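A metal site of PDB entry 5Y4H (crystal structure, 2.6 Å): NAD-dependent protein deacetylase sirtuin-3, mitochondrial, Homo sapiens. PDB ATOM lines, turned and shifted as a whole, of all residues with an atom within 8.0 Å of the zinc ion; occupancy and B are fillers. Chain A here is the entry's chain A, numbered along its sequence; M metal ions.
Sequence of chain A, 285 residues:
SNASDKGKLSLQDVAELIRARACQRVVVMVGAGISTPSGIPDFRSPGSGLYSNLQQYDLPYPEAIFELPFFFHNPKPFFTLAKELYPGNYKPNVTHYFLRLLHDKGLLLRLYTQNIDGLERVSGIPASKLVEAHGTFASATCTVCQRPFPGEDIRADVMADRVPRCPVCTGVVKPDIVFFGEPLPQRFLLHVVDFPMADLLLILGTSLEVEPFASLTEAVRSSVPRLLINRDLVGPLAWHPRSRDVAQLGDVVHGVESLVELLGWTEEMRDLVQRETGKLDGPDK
The side-chain sulfur of Cys 166 sits close to the backbone NH of Val 168, 3.5 Å away.
SG of Cys 145 lies close to N of Arg 147 (3.6 Å).
The backbone NH of Gly 171 sits close to the side-chain sulfur of Cys 169, 3.6 Å away.
The backbone NH of Cys 166 lies within hydrogen-bond range of the backbone carbonyl oxygen of Gly 171, at 2.8 Å.
The backbone NH of Val 144 sits close to the side-chain sulfur of Cys 142, 3.4 Å away.
N of Cys 142 lies within hydrogen-bond range of O of Arg 147.
Within 4 Å of the zinc ion: Cys 142, Cys 145, Cys 166 and Cys 169.
The zinc ion is bound by the side-chain sulfur of Cys 145, the side-chain sulfur of Cys 166, the side-chain sulfur of Cys 142 and the side-chain sulfur of Cys 169.
The zinc ion has four donor atoms within binding distance.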
ATOM      1  N   THR A 141      28.883  16.994  -0.255  1.00  0.00           N
ATOM      2  CA  THR A 141      28.024  15.830  -0.141  1.00  0.00           C
ATOM      3  C   THR A 141      27.259  15.623  -1.443  1.00  0.00           C
ATOM      4  O   THR A 141      26.688  16.578  -1.989  1.00  0.00           O
ATOM      5  CB  THR A 141      27.000  15.981   1.018  1.00  0.00           C
ATOM      6  OG1 THR A 141      27.650  16.463   2.199  1.00  0.00           O
ATOM      7  CG2 THR A 141      26.316  14.657   1.332  1.00  0.00           C
ATOM      8  N   CYS A 142      27.247  14.388  -1.923  1.00  0.00           N
ATOM      9  CA  CYS A 142      26.368  14.046  -3.025  1.00  0.00           C
ATOM     10  C   CYS A 142      24.919  14.244  -2.573  1.00  0.00           C
ATOM     11  O   CYS A 142      24.455  13.588  -1.636  1.00  0.00           O
ATOM     12  CB  CYS A 142      26.600  12.619  -3.529  1.00  0.00           C
ATOM     13  SG  CYS A 142      25.343  12.039  -4.713  1.00  0.00           S
ATOM     14  N   THR A 143      24.245  15.162  -3.249  1.00  0.00           N
ATOM     15  CA  THR A 143      22.829  15.465  -3.039  1.00  0.00           C
ATOM     16  C   THR A 143      21.873  14.282  -3.155  1.00  0.00           C
ATOM     17  O   THR A 143      20.721  14.398  -2.729  1.00  0.00           O
ATOM     18  CB  THR A 143      22.344  16.530  -4.047  1.00  0.00           C
ATOM     19  OG1 THR A 143      22.542  16.046  -5.394  1.00  0.00           O
ATOM     20  CG2 THR A 143      23.075  17.851  -3.831  1.00  0.00           C
ATOM     21  N   VAL A 144      22.334  13.183  -3.744  1.00  0.00           N
ATOM     22  CA  VAL A 144      21.475  12.005  -3.974  1.00  0.00           C
ATOM     23  C   VAL A 144      21.738  10.881  -2.939  1.00  0.00           C
ATOM     24  O   VAL A 144      20.859  10.594  -2.117  1.00  0.00           O
ATOM     25  CB  VAL A 144      21.538  11.499  -5.445  1.00  0.00           C
ATOM     26  CG1 VAL A 144      20.729  10.234  -5.637  1.00  0.00           C
ATOM     27  CG2 VAL A 144      21.040  12.558  -6.401  1.00  0.00           C
ATOM     28  N   CYS A 145      22.931  10.275  -2.984  1.00  0.00           N
ATOM     29  CA  CYS A 145      23.249   9.132  -2.110  1.00  0.00           C
ATOM     30  C   CYS A 145      23.810   9.554  -0.748  1.00  0.00           C
ATOM     31  O   CYS A 145      23.862   8.740   0.171  1.00  0.00           O
ATOM     32  CB  CYS A 145      24.207   8.162  -2.799  1.00  0.00           C
ATOM     33  SG  CYS A 145      25.896   8.780  -2.915  1.00  0.00           S
ATOM     34  N   GLN A 146      24.227  10.824  -0.655  1.00  0.00           N
ATOM     35  CA  GLN A 146      24.734  11.462   0.575  1.00  0.00           C
ATOM     36  C   GLN A 146      26.123  11.014   0.997  1.00  0.00           C
ATOM     37  O   GLN A 146      26.457  11.078   2.188  1.00  0.00           O
ATOM     38  CB  GLN A 146      23.748  11.335   1.733  1.00  0.00           C
ATOM     39  CG  GLN A 146      22.386  11.935   1.488  1.00  0.00           C
ATOM     40  CD  GLN A 146      21.507  11.751   2.689  1.00  0.00           C
ATOM     41  OE1 GLN A 146      21.850  12.179   3.788  1.00  0.00           O
ATOM     42  NE2 GLN A 146      20.371  11.083   2.505  1.00  0.00           N
ATOM     43  N   ARG A 147      26.914  10.577   0.036  1.00  0.00           N
ATOM     44  CA  ARG A 147      28.314  10.269   0.252  1.00  0.00           C
ATOM     45  C   ARG A 147      29.113  11.577   0.508  1.00  0.00           C
ATOM     46  O   ARG A 147      28.895  12.571  -0.186  1.00  0.00           O
ATOM     47  CB  ARG A 147      28.848   9.440  -0.927  1.00  0.00           C
ATOM     48  CG  ARG A 147      30.351   9.533  -1.209  1.00  0.00           C
ATOM     49  CD  ARG A 147      30.705   8.794  -2.480  1.00  0.00           C
ATOM     50  NE  ARG A 147      31.595   7.660  -2.239  1.00  0.00           N
ATOM     51  CZ  ARG A 147      32.832   7.542  -2.718  1.00  0.00           C
ATOM     52  NH1 ARG A 147      33.369   8.481  -3.498  1.00  0.00           N
ATOM     53  NH2 ARG A 147      33.546   6.466  -2.420  1.00  0.00           N
ATOM     54  N   PRO A 148      30.009  11.574   1.517  1.00  0.00           N
ATOM     55  CA  PRO A 148      30.846  12.744   1.801  1.00  0.00           C
ATOM     56  C   PRO A 148      32.105  12.821   0.946  1.00  0.00           C
ATOM     57  O   PRO A 148      32.712  11.805   0.645  1.00  0.00           O
ATOM     58  CB  PRO A 148      31.210  12.548   3.267  1.00  0.00           C
ATOM     59  CG  PRO A 148      31.251  11.068   3.443  1.00  0.00           C
ATOM     60  CD  PRO A 148      30.227  10.497   2.500  1.00  0.00           C
ATOM     61  N   PHE A 149      32.481  14.039   0.567  1.00  0.00           N
ATOM     62  CA  PHE A 149      33.645  14.304  -0.295  1.00  0.00           C
ATOM     63  C   PHE A 149      34.582  15.332   0.340  1.00  0.00           C
ATOM     64  O   PHE A 149      34.116  16.296   0.952  1.00  0.00           O
ATOM     65  CB  PHE A 149      33.198  14.834  -1.651  1.00  0.00           C
ATOM     66  CG  PHE A 149      32.495  13.821  -2.510  1.00  0.00           C
ATOM     67  CD1 PHE A 149      33.218  13.010  -3.391  1.00  0.00           C
ATOM     68  CD2 PHE A 149      31.097  13.671  -2.448  1.00  0.00           C
ATOM     69  CE1 PHE A 149      32.565  12.061  -4.182  1.00  0.00           C
ATOM     70  CE2 PHE A 149      30.442  12.732  -3.239  1.00  0.00           C
ATOM     71  CZ  PHE A 149      31.175  11.932  -4.111  1.00  0.00           C
ATOM     72  N   ARG A 165      29.940  15.624 -10.188  1.00  0.00           N
ATOM     73  CA  ARG A 165      28.993  14.520 -10.120  1.00  0.00           C
ATOM     74  C   ARG A 165      29.562  13.342  -9.332  1.00  0.00           C
ATOM     75  O   ARG A 165      30.772  13.128  -9.277  1.00  0.00           O
ATOM     76  CB  ARG A 165      28.515  14.124 -11.521  1.00  0.00           C
ATOM     77  CG  ARG A 165      27.763  15.235 -12.237  1.00  0.00           C
ATOM     78  CD  ARG A 165      26.680  14.715 -13.169  1.00  0.00           C
ATOM     79  NE  ARG A 165      25.755  15.791 -13.519  1.00  0.00           N
ATOM     80  CZ  ARG A 165      24.470  15.860 -13.158  1.00  0.00           C
ATOM     81  NH1 ARG A 165      23.733  16.887 -13.546  1.00  0.00           N
ATOM     82  NH2 ARG A 165      23.920  14.901 -12.427  1.00  0.00           N
ATOM     83  N   CYS A 166      28.666  12.609  -8.684  1.00  0.00           N
ATOM     84  CA  CYS A 166      29.040  11.532  -7.763  1.00  0.00           C
ATOM     85  C   CYS A 166      29.584  10.307  -8.521  1.00  0.00           C
ATOM     86  O   CYS A 166      28.884   9.761  -9.375  1.00  0.00           O
ATOM     87  CB  CYS A 166      27.843  11.169  -6.891  1.00  0.00           C
ATOM     88  SG  CYS A 166      28.092   9.828  -5.705  1.00  0.00           S
ATOM     89  N   PRO A 167      30.831   9.886  -8.209  1.00  0.00           N
ATOM     90  CA  PRO A 167      31.424   8.652  -8.752  1.00  0.00           C
ATOM     91  C   PRO A 167      30.525   7.420  -8.636  1.00  0.00           C
ATOM     92  O   PRO A 167      30.661   6.509  -9.442  1.00  0.00           O
ATOM     93  CB  PRO A 167      32.665   8.441  -7.882  1.00  0.00           C
ATOM     94  CG  PRO A 167      33.075   9.807  -7.479  1.00  0.00           C
ATOM     95  CD  PRO A 167      31.809  10.631  -7.392  1.00  0.00           C
ATOM     96  N   VAL A 168      29.630   7.412  -7.645  1.00  0.00           N
ATOM     97  CA  VAL A 168      28.832   6.232  -7.317  1.00  0.00           C
ATOM     98  C   VAL A 168      27.376   6.298  -7.822  1.00  0.00           C
ATOM     99  O   VAL A 168      26.730   5.259  -7.953  1.00  0.00           O
ATOM    100  CB  VAL A 168      28.880   5.888  -5.796  1.00  0.00           C
ATOM    101  CG1 VAL A 168      28.615   4.404  -5.548  1.00  0.00           C
ATOM    102  CG2 VAL A 168      30.235   6.254  -5.183  1.00  0.00           C
ATOM    103  N   CYS A 169      26.864   7.499  -8.131  1.00  0.00           N
ATOM    104  CA  CYS A 169      25.456   7.639  -8.558  1.00  0.00           C
ATOM    105  C   CYS A 169      25.126   8.778  -9.532  1.00  0.00           C
ATOM    106  O   CYS A 169      23.976   8.909  -9.954  1.00  0.00           O
ATOM    107  CB  CYS A 169      24.531   7.689  -7.327  1.00  0.00           C
ATOM    108  SG  CYS A 169      24.321   9.335  -6.591  1.00  0.00           S
ATOM    109  N   THR A 170      26.128   9.578  -9.898  1.00  0.00           N
ATOM    110  CA  THR A 170      25.995  10.680 -10.901  1.00  0.00           C
ATOM    111  C   THR A 170      25.192  11.896 -10.431  1.00  0.00           C
ATOM    112  O   THR A 170      25.011  12.850 -11.203  1.00  0.00           O
ATOM    113  CB  THR A 170      25.452  10.243 -12.306  1.00  0.00           C
ATOM    114  OG1 THR A 170      25.208   8.826 -12.360  1.00  0.00           O
ATOM    115  CG2 THR A 170      26.413  10.668 -13.425  1.00  0.00           C
ATOM    116  N   GLY A 171      24.702  11.862  -9.183  1.00  0.00           N
ATOM    117  CA  GLY A 171      24.051  13.019  -8.556  1.00  0.00           C
ATOM    118  C   GLY A 171      25.012  14.191  -8.421  1.00  0.00           C
ATOM    119  O   GLY A 171      26.244  13.997  -8.327  1.00  0.00           O
ATOM    120  N   VAL A 172      24.462  15.414  -8.440  1.00  0.00           N
ATOM    121  CA  VAL A 172      25.279  16.629  -8.253  1.00  0.00           C
ATOM    122  C   VAL A 172      25.923  16.577  -6.878  1.00  0.00           C
ATOM    123  O   VAL A 172      25.276  16.263  -5.877  1.00  0.00           O
ATOM    124  CB  VAL A 172      24.466  17.935  -8.454  1.00  0.00           C
ATOM    125  CG1 VAL A 172      25.313  19.168  -8.169  1.00  0.00           C
ATOM    126  CG2 VAL A 172      23.924  18.017  -9.872  1.00  0.00           C
ATOM    127  N   VAL A 173      27.228  16.867  -6.839  1.00  0.00           N
ATOM    128  CA  VAL A 173      27.984  16.955  -5.603  1.00  0.00           C
ATOM    129  C   VAL A 173      28.016  18.427  -5.132  1.00  0.00           C
ATOM    130  O   VAL A 173      28.788  19.254  -5.657  1.00  0.00           O
ATOM    131  CB  VAL A 173      29.389  16.332  -5.768  1.00  0.00           C
ATOM    132  CG1 VAL A 173      30.235  16.504  -4.510  1.00  0.00           C
ATOM    133  CG2 VAL A 173      29.264  14.853  -6.095  1.00  0.00           C
HETATM  134 ZN    ZN M   1      26.013   9.812  -4.866  1.00  0.00          ZN
